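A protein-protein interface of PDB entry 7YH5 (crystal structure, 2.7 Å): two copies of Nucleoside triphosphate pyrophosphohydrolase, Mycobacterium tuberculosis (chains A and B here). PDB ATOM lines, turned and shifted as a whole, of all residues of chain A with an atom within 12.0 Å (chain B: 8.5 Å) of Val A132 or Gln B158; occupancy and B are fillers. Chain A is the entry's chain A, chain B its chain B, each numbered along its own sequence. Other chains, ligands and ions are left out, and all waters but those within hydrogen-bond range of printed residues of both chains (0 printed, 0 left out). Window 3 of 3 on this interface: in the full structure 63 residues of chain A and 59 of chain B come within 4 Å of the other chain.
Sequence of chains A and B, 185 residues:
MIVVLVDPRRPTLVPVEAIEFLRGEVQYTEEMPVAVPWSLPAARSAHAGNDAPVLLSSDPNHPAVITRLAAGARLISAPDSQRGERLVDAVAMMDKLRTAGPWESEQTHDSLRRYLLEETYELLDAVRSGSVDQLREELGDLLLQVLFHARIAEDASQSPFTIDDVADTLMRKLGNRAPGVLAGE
Printed residues of chain B that touch a printed residue of chain A: His B109, Gln B158, Ser B159, Phe B161 and Thr B169. Hydrophobic or aromatic side chains of chain B that line the printed part of chain A: His B109 and Phe B161. Of the 20 printed residues of chain A, 5 touch a printed residue of chain B. Hydrophobic or aromatic side chains of chain A that line the printed part of chain B: Val A127, Val A132 and Leu A135. Along chain A the printed residues that touch a printed residue of chain B span positions 127 to 137. Among the printed residues, no Asp or Glu carboxylate lies within 4 Å of a Lys or Arg side-chain nitrogen of the other chain.
No position is printed for both chains.
O of His B109 touches CG1 of Val A127, at 3.8 Å. Val A132 touches Gln B158 (CG1 to OE1, 3.7 Å). CB of Ser B159 touches CG2 of Val A132, 3.7 Å away. Phe B161 touches Val A132. Leu A135 touches His B109. Leu A135 touches Phe B161 (CD2 to CZ, 3.9 Å). Phe B161 touches Arg A136. Arg A136 touches Thr B169. Thr B169 touches Glu A137.
Gly A130 touches none of the printed residues of chain B. Asp A133 touches none of the printed residues of chain B. Of the printed residues of chain B, Arg A136 touches Phe B161 and Thr B169. Printed residues of chain A within 4 Å of His B109: Val A127 and Leu A135. No residue of chain A comes within 4 Å of Ala B156. No residue of chain A comes within 4 Å of Ser B157. Gln B158 touches just one residue of chain A: Val A132 (3.7 Å). Ser B159 touches one residue of chain A. No residue of chain A comes within 4 Å of Pro B160. Printed residues of chain A within 4 Å of Thr B169: Arg A136 and Glu A137. The nearest residue of chain B that does not touch Val A132 is Ala B156 (6.0 Å). The nearest residue of chain A that does not touch Gln B158 is Gly A130 (5.2 Å).
The backbone carbonyl oxygen (O) of Ala B153 sits at hydrogen-bond distance from the backbone NH (N) of Phe B161 (3.2 Å). The backbone carbonyl oxygen of Phe B161 is in hydrogen-bond range of the backbone NH of Glu B154 (3.2 Å).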
ATOM      1  N   GLU A 122     -14.569  33.476  -3.417  1.00  0.00           N
ATOM      2  CA  GLU A 122     -15.172  32.928  -4.628  1.00  0.00           C
ATOM      3  C   GLU A 122     -16.449  32.156  -4.319  1.00  0.00           C
ATOM      4  O   GLU A 122     -17.388  32.168  -5.124  1.00  0.00           O
ATOM      5  CB  GLU A 122     -14.166  32.036  -5.357  1.00  0.00           C
ATOM      6  CG  GLU A 122     -12.983  32.799  -5.936  1.00  0.00           C
ATOM      7  CD  GLU A 122     -12.048  31.915  -6.736  1.00  0.00           C
ATOM      8  OE1 GLU A 122     -10.973  32.401  -7.148  1.00  0.00           O
ATOM      9  OE2 GLU A 122     -12.389  30.734  -6.953  1.00  0.00           O
ATOM     10  N   LEU A 123     -16.505  31.475  -3.170  1.00  0.00           N
ATOM     11  CA  LEU A 123     -17.733  30.791  -2.776  1.00  0.00           C
ATOM     12  C   LEU A 123     -18.862  31.788  -2.548  1.00  0.00           C
ATOM     13  O   LEU A 123     -19.998  31.568  -2.984  1.00  0.00           O
ATOM     14  CB  LEU A 123     -17.494  29.950  -1.520  1.00  0.00           C
ATOM     15  CG  LEU A 123     -18.738  29.250  -0.969  1.00  0.00           C
ATOM     16  CD1 LEU A 123     -19.375  28.384  -2.043  1.00  0.00           C
ATOM     17  CD2 LEU A 123     -18.407  28.422   0.262  1.00  0.00           C
ATOM     18  N   LEU A 124     -18.565  32.890  -1.853  1.00  0.00           N
ATOM     19  CA  LEU A 124     -19.561  33.941  -1.675  1.00  0.00           C
ATOM     20  C   LEU A 124     -20.007  34.491  -3.023  1.00  0.00           C
ATOM     21  O   LEU A 124     -21.191  34.788  -3.223  1.00  0.00           O
ATOM     22  CB  LEU A 124     -19.005  35.055  -0.787  1.00  0.00           C
ATOM     23  CG  LEU A 124     -18.854  34.731   0.703  1.00  0.00           C
ATOM     24  CD1 LEU A 124     -18.160  35.868   1.431  1.00  0.00           C
ATOM     25  CD2 LEU A 124     -20.204  34.434   1.338  1.00  0.00           C
ATOM     26  N   ASP A 125     -19.065  34.638  -3.962  1.00  0.00           N
ATOM     27  CA  ASP A 125     -19.416  35.072  -5.309  1.00  0.00           C
ATOM     28  C   ASP A 125     -20.369  34.093  -5.980  1.00  0.00           C
ATOM     29  O   ASP A 125     -21.223  34.503  -6.775  1.00  0.00           O
ATOM     30  CB  ASP A 125     -18.149  35.218  -6.155  1.00  0.00           C
ATOM     31  CG  ASP A 125     -17.371  36.479  -5.835  1.00  0.00           C
ATOM     32  OD1 ASP A 125     -17.746  37.189  -4.880  1.00  0.00           O
ATOM     33  OD2 ASP A 125     -16.373  36.752  -6.538  1.00  0.00           O
ATOM     34  N   ALA A 126     -20.244  32.800  -5.676  1.00  0.00           N
ATOM     35  CA  ALA A 126     -21.132  31.806  -6.266  1.00  0.00           C
ATOM     36  C   ALA A 126     -22.520  31.831  -5.640  1.00  0.00           C
ATOM     37  O   ALA A 126     -23.506  31.520  -6.318  1.00  0.00           O
ATOM     38  CB  ALA A 126     -20.523  30.408  -6.135  1.00  0.00           C
ATOM     39  N   VAL A 127     -22.618  32.197  -4.360  1.00  0.00           N
ATOM     40  CA  VAL A 127     -23.915  32.214  -3.689  1.00  0.00           C
ATOM     41  C   VAL A 127     -24.779  33.344  -4.232  1.00  0.00           C
ATOM     42  O   VAL A 127     -25.948  33.142  -4.581  1.00  0.00           O
ATOM     43  CB  VAL A 127     -23.728  32.326  -2.165  1.00  0.00           C
ATOM     44  CG1 VAL A 127     -25.078  32.434  -1.470  1.00  0.00           C
ATOM     45  CG2 VAL A 127     -22.949  31.132  -1.639  1.00  0.00           C
ATOM     46  N   ARG A 128     -24.215  34.548  -4.320  1.00  0.00           N
ATOM     47  CA  ARG A 128     -24.913  35.700  -4.872  1.00  0.00           C
ATOM     48  C   ARG A 128     -24.943  35.698  -6.398  1.00  0.00           C
ATOM     49  O   ARG A 128     -25.317  36.714  -6.996  1.00  0.00           O
ATOM     50  CB  ARG A 128     -24.276  36.994  -4.362  1.00  0.00           C
ATOM     51  N   SER A 129     -24.551  34.591  -7.033  1.00  0.00           N
ATOM     52  CA  SER A 129     -24.671  34.431  -8.475  1.00  0.00           C
ATOM     53  C   SER A 129     -25.797  33.495  -8.887  1.00  0.00           C
ATOM     54  O   SER A 129     -26.252  33.574 -10.033  1.00  0.00           O
ATOM     55  CB  SER A 129     -23.356  33.908  -9.072  1.00  0.00           C
ATOM     56  OG  SER A 129     -23.164  32.536  -8.770  1.00  0.00           O
ATOM     57  N   GLY A 130     -26.251  32.618  -7.993  1.00  0.00           N
ATOM     58  CA  GLY A 130     -27.310  31.683  -8.288  1.00  0.00           C
ATOM     59  C   GLY A 130     -26.869  30.393  -8.949  1.00  0.00           C
ATOM     60  O   GLY A 130     -27.573  29.384  -8.830  1.00  0.00           O
ATOM     61  N   SER A 131     -25.726  30.393  -9.637  1.00  0.00           N
ATOM     62  CA  SER A 131     -25.261  29.230 -10.384  1.00  0.00           C
ATOM     63  C   SER A 131     -25.024  28.030  -9.473  1.00  0.00           C
ATOM     64  O   SER A 131     -24.115  28.051  -8.638  1.00  0.00           O
ATOM     65  CB  SER A 131     -23.980  29.572 -11.146  1.00  0.00           C
ATOM     66  OG  SER A 131     -23.445  28.422 -11.775  1.00  0.00           O
ATOM     67  N   VAL A 132     -25.831  26.975  -9.632  1.00  0.00           N
ATOM     68  CA  VAL A 132     -25.674  25.787  -8.795  1.00  0.00           C
ATOM     69  C   VAL A 132     -24.381  25.046  -9.118  1.00  0.00           C
ATOM     70  O   VAL A 132     -23.747  24.471  -8.224  1.00  0.00           O
ATOM     71  CB  VAL A 132     -26.897  24.861  -8.938  1.00  0.00           C
ATOM     72  CG1 VAL A 132     -28.101  25.463  -8.231  1.00  0.00           C
ATOM     73  CG2 VAL A 132     -27.213  24.603 -10.409  1.00  0.00           C
ATOM     74  N   ASP A 133     -23.970  25.036 -10.390  1.00  0.00           N
ATOM     75  CA  ASP A 133     -22.754  24.329 -10.780  1.00  0.00           C
ATOM     76  C   ASP A 133     -21.506  25.008 -10.236  1.00  0.00           C
ATOM     77  O   ASP A 133     -20.498  24.336  -9.982  1.00  0.00           O
ATOM     78  CB  ASP A 133     -22.678  24.205 -12.306  1.00  0.00           C
ATOM     79  CG  ASP A 133     -23.847  23.430 -12.888  1.00  0.00           C
ATOM     80  OD1 ASP A 133     -24.344  23.796 -13.977  1.00  0.00           O
ATOM     81  OD2 ASP A 133     -24.287  22.463 -12.231  1.00  0.00           O
ATOM     82  N   GLN A 134     -21.551  26.327 -10.053  1.00  0.00           N
ATOM     83  CA  GLN A 134     -20.453  27.041  -9.418  1.00  0.00           C
ATOM     84  C   GLN A 134     -20.532  27.005  -7.899  1.00  0.00           C
ATOM     85  O   GLN A 134     -19.490  27.043  -7.233  1.00  0.00           O
ATOM     86  CB  GLN A 134     -20.415  28.496  -9.891  1.00  0.00           C
ATOM     87  CG  GLN A 134     -19.746  28.686 -11.242  1.00  0.00           C
ATOM     88  CD  GLN A 134     -19.774  30.127 -11.706  1.00  0.00           C
ATOM     89  OE1 GLN A 134     -20.292  31.003 -11.014  1.00  0.00           O
ATOM     90  NE2 GLN A 134     -19.221  30.378 -12.887  1.00  0.00           N
ATOM     91  N   LEU A 135     -21.738  26.947  -7.331  1.00  0.00           N
ATOM     92  CA  LEU A 135     -21.856  26.771  -5.888  1.00  0.00           C
ATOM     93  C   LEU A 135     -21.280  25.429  -5.463  1.00  0.00           C
ATOM     94  O   LEU A 135     -20.536  25.340  -4.481  1.00  0.00           O
ATOM     95  CB  LEU A 135     -23.314  26.893  -5.450  1.00  0.00           C
ATOM     96  CG  LEU A 135     -23.521  26.662  -3.951  1.00  0.00           C
ATOM     97  CD1 LEU A 135     -22.837  27.760  -3.148  1.00  0.00           C
ATOM     98  CD2 LEU A 135     -24.998  26.568  -3.592  1.00  0.00           C
ATOM     99  N   ARG A 136     -21.607  24.367  -6.206  1.00  0.00           N
ATOM    100  CA  ARG A 136     -21.058  23.054  -5.893  1.00  0.00           C
ATOM    101  C   ARG A 136     -19.556  23.000  -6.145  1.00  0.00           C
ATOM    102  O   ARG A 136     -18.837  22.290  -5.434  1.00  0.00           O
ATOM    103  CB  ARG A 136     -21.773  21.976  -6.707  1.00  0.00           C
ATOM    104  N   GLU A 137     -19.067  23.740  -7.142  1.00  0.00           N
ATOM    105  CA  GLU A 137     -17.637  23.736  -7.430  1.00  0.00           C
ATOM    106  C   GLU A 137     -16.856  24.450  -6.336  1.00  0.00           C
ATOM    107  O   GLU A 137     -15.851  23.930  -5.835  1.00  0.00           O
ATOM    108  CB  GLU A 137     -17.370  24.378  -8.791  1.00  0.00           C
ATOM    109  CG  GLU A 137     -16.009  24.022  -9.363  1.00  0.00           C
ATOM    110  CD  GLU A 137     -15.717  24.718 -10.676  1.00  0.00           C
ATOM    111  OE1 GLU A 137     -14.543  25.073 -10.909  1.00  0.00           O
ATOM    112  OE2 GLU A 137     -16.658  24.905 -11.477  1.00  0.00           O
ATOM    113  N   GLU A 138     -17.299  25.649  -5.950  1.00  0.00           N
ATOM    114  CA  GLU A 138     -16.605  26.390  -4.904  1.00  0.00           C
ATOM    115  C   GLU A 138     -16.788  25.761  -3.530  1.00  0.00           C
ATOM    116  O   GLU A 138     -15.999  26.046  -2.623  1.00  0.00           O
ATOM    117  CB  GLU A 138     -17.067  27.848  -4.892  1.00  0.00           C
ATOM    118  CG  GLU A 138     -16.537  28.653  -6.064  1.00  0.00           C
ATOM    119  CD  GLU A 138     -15.064  28.395  -6.317  1.00  0.00           C
ATOM    120  OE1 GLU A 138     -14.273  28.469  -5.355  1.00  0.00           O
ATOM    121  OE2 GLU A 138     -14.699  28.101  -7.474  1.00  0.00           O
ATOM    122  N   LEU A 139     -17.808  24.919  -3.353  1.00  0.00           N
ATOM    123  CA  LEU A 139     -17.920  24.156  -2.115  1.00  0.00           C
ATOM    124  C   LEU A 139     -16.821  23.105  -2.022  1.00  0.00           C
ATOM    125  O   LEU A 139     -16.230  22.908  -0.953  1.00  0.00           O
ATOM    126  CB  LEU A 139     -19.302  23.507  -2.018  1.00  0.00           C
ATOM    127  CG  LEU A 139     -20.408  24.388  -1.433  1.00  0.00           C
ATOM    128  CD1 LEU A 139     -21.693  23.599  -1.223  1.00  0.00           C
ATOM    129  CD2 LEU A 139     -19.950  25.030  -0.135  1.00  0.00           C
ATOM    130  N   GLY A 140     -16.533  22.421  -3.131  1.00  0.00           N
ATOM    131  CA  GLY A 140     -15.428  21.479  -3.147  1.00  0.00           C
ATOM    132  C   GLY A 140     -14.079  22.138  -2.977  1.00  0.00           C
ATOM    133  O   GLY A 140     -13.172  21.554  -2.378  1.00  0.00           O
ATOM    134  N   ASP A 141     -13.923  23.354  -3.502  1.00  0.00           N
ATOM    135  CA  ASP A 141     -12.671  24.076  -3.320  1.00  0.00           C
ATOM    136  C   ASP A 141     -12.443  24.424  -1.854  1.00  0.00           C
ATOM    137  O   ASP A 141     -11.320  24.311  -1.351  1.00  0.00           O
ATOM    138  CB  ASP A 141     -12.662  25.331  -4.191  1.00  0.00           C
ATOM    139  CG  ASP A 141     -12.297  25.032  -5.635  1.00  0.00           C
ATOM    140  OD1 ASP A 141     -11.733  23.947  -5.895  1.00  0.00           O
ATOM    141  OD2 ASP A 141     -12.573  25.880  -6.510  1.00  0.00           O
ATOM    142  N   HIS B 109     -28.851  29.503   1.849  1.00  0.00           N
ATOM    143  CA  HIS B 109     -27.483  29.801   1.434  1.00  0.00           C
ATOM    144  C   HIS B 109     -27.105  31.244   1.749  1.00  0.00           C
ATOM    145  O   HIS B 109     -25.955  31.527   2.108  1.00  0.00           O
ATOM    146  CB  HIS B 109     -27.321  29.510  -0.057  1.00  0.00           C
ATOM    147  CG  HIS B 109     -27.336  28.050  -0.389  1.00  0.00           C
ATOM    148  ND1 HIS B 109     -27.898  27.553  -1.545  1.00  0.00           N
ATOM    149  CD2 HIS B 109     -26.862  26.978   0.289  1.00  0.00           C
ATOM    150  CE1 HIS B 109     -27.769  26.238  -1.565  1.00  0.00           C
ATOM    151  NE2 HIS B 109     -27.141  25.864  -0.465  1.00  0.00           N
ATOM    152  N   ALA B 153     -28.499  22.178  -0.181  1.00  0.00           N
ATOM    153  CA  ALA B 153     -28.639  21.949  -1.615  1.00  0.00           C
ATOM    154  C   ALA B 153     -29.397  20.670  -1.937  1.00  0.00           C
ATOM    155  O   ALA B 153     -29.829  20.501  -3.082  1.00  0.00           O
ATOM    156  CB  ALA B 153     -27.263  21.916  -2.280  1.00  0.00           C
ATOM    157  N   GLU B 154     -29.557  19.763  -0.971  1.00  0.00           N
ATOM    158  CA  GLU B 154     -30.440  18.621  -1.172  1.00  0.00           C
ATOM    159  C   GLU B 154     -31.882  19.081  -1.343  1.00  0.00           C
ATOM    160  O   GLU B 154     -32.605  18.604  -2.225  1.00  0.00           O
ATOM    161  CB  GLU B 154     -30.327  17.656   0.009  1.00  0.00           C
ATOM    162  CG  GLU B 154     -28.934  17.092   0.250  1.00  0.00           C
ATOM    163  CD  GLU B 154     -28.958  15.809   1.063  1.00  0.00           C
ATOM    164  OE1 GLU B 154     -30.044  15.204   1.184  1.00  0.00           O
ATOM    165  OE2 GLU B 154     -27.895  15.407   1.582  1.00  0.00           O
ATOM    166  N   ASP B 155     -32.294  20.020  -0.485  1.00  0.00           N
ATOM    167  CA  ASP B 155     -33.676  20.573  -0.513  1.00  0.00           C
ATOM    168  C   ASP B 155     -33.854  21.438  -1.766  1.00  0.00           C
ATOM    169  O   ASP B 155     -34.959  21.986  -1.952  1.00  0.00           O
ATOM    170  CB  ASP B 155     -33.986  21.359   0.764  1.00  0.00           C
ATOM    171  CG  ASP B 155     -33.934  20.510   2.022  1.00  0.00           C
ATOM    172  OD1 ASP B 155     -34.004  19.272   1.896  1.00  0.00           O
ATOM    173  OD2 ASP B 155     -33.825  21.095   3.119  1.00  0.00           O
ATOM    174  N   ALA B 156     -32.804  21.548  -2.587  1.00  0.00           N
ATOM    175  CA  ALA B 156     -32.861  22.357  -3.828  1.00  0.00           C
ATOM    176  C   ALA B 156     -34.010  21.862  -4.714  1.00  0.00           C
ATOM    177  O   ALA B 156     -34.144  20.632  -4.877  1.00  0.00           O
ATOM    178  CB  ALA B 156     -31.537  22.289  -4.547  1.00  0.00           C
ATOM    179  N   SER B 157     -34.800  22.790  -5.261  1.00  0.00           N
ATOM    180  CA  SER B 157     -35.947  22.436  -6.137  1.00  0.00           C
ATOM    181  C   SER B 157     -35.476  22.326  -7.593  1.00  0.00           C
ATOM    182  O   SER B 157     -36.215  21.743  -8.411  1.00  0.00           O
ATOM    183  CB  SER B 157     -37.065  23.437  -5.996  1.00  0.00           C
ATOM    184  OG  SER B 157     -37.492  23.528  -4.646  1.00  0.00           O
ATOM    185  N   GLN B 158     -34.291  22.868  -7.891  1.00  0.00           N
ATOM    186  CA  GLN B 158     -33.728  22.822  -9.268  1.00  0.00           C
ATOM    187  C   GLN B 158     -32.253  22.411  -9.199  1.00  0.00           C
ATOM    188  O   GLN B 158     -31.483  23.087  -8.487  1.00  0.00           O
ATOM    189  CB  GLN B 158     -33.893  24.177  -9.958  1.00  0.00           C
ATOM    190  CG  GLN B 158     -33.619  25.365  -9.047  1.00  0.00           C
ATOM    191  CD  GLN B 158     -32.150  25.705  -8.980  1.00  0.00           C
ATOM    192  OE1 GLN B 158     -31.375  25.380  -9.877  1.00  0.00           O
ATOM    193  NE2 GLN B 158     -31.754  26.367  -7.905  1.00  0.00           N
ATOM    194  N   SER B 159     -31.886  21.343  -9.913  1.00  0.00           N
ATOM    195  CA  SER B 159     -30.486  20.843  -9.934  1.00  0.00           C
ATOM    196  C   SER B 159     -29.970  20.669  -8.500  1.00  0.00           C
ATOM    197  O   SER B 159     -28.928  21.267  -8.170  1.00  0.00           O
ATOM    198  CB  SER B 159     -29.595  21.760 -10.731  1.00  0.00           C
ATOM    199  OG  SER B 159     -30.280  22.267 -11.867  1.00  0.00           O
ATOM    200  N   PRO B 160     -30.650  19.880  -7.638  1.00  0.00           N
ATOM    201  CA  PRO B 160     -30.202  19.673  -6.258  1.00  0.00           C
ATOM    202  C   PRO B 160     -29.016  18.698  -6.205  1.00  0.00           C
ATOM    203  O   PRO B 160     -28.980  17.780  -7.006  1.00  0.00           O
ATOM    204  CB  PRO B 160     -31.432  19.046  -5.586  1.00  0.00           C
ATOM    205  CG  PRO B 160     -32.119  18.300  -6.709  1.00  0.00           C
ATOM    206  CD  PRO B 160     -31.882  19.148  -7.943  1.00  0.00           C
ATOM    207  N   PHE B 161     -28.086  18.922  -5.271  1.00  0.00           N
ATOM    208  CA  PHE B 161     -26.893  18.044  -5.133  1.00  0.00           C
ATOM    209  C   PHE B 161     -26.669  17.700  -3.655  1.00  0.00           C
ATOM    210  O   PHE B 161     -27.328  18.300  -2.783  1.00  0.00           O
ATOM    211  CB  PHE B 161     -25.659  18.713  -5.746  1.00  0.00           C
ATOM    212  CG  PHE B 161     -25.386  20.112  -5.253  1.00  0.00           C
ATOM    213  CD1 PHE B 161     -25.883  21.214  -5.931  1.00  0.00           C
ATOM    214  CD2 PHE B 161     -24.631  20.329  -4.111  1.00  0.00           C
ATOM    215  CE1 PHE B 161     -25.631  22.499  -5.478  1.00  0.00           C
ATOM    216  CE2 PHE B 161     -24.380  21.614  -3.659  1.00  0.00           C
ATOM    217  CZ  PHE B 161     -24.880  22.697  -4.343  1.00  0.00           C
ATOM    218  N   THR B 169     -17.013  16.477  -7.295  1.00  0.00           N
ATOM    219  CA  THR B 169     -16.532  17.688  -7.953  1.00  0.00           C
ATOM    220  C   THR B 169     -15.076  17.962  -7.597  1.00  0.00           C
ATOM    221  O   THR B 169     -14.248  18.231  -8.475  1.00  0.00           O
ATOM    222  CB  THR B 169     -17.412  18.877  -7.566  1.00  0.00           C
ATOM    223  OG1 THR B 169     -18.717  18.714  -8.133  1.00  0.00           O
ATOM    224  CG2 THR B 169     -16.802  20.182  -8.063  1.00  0.00           C
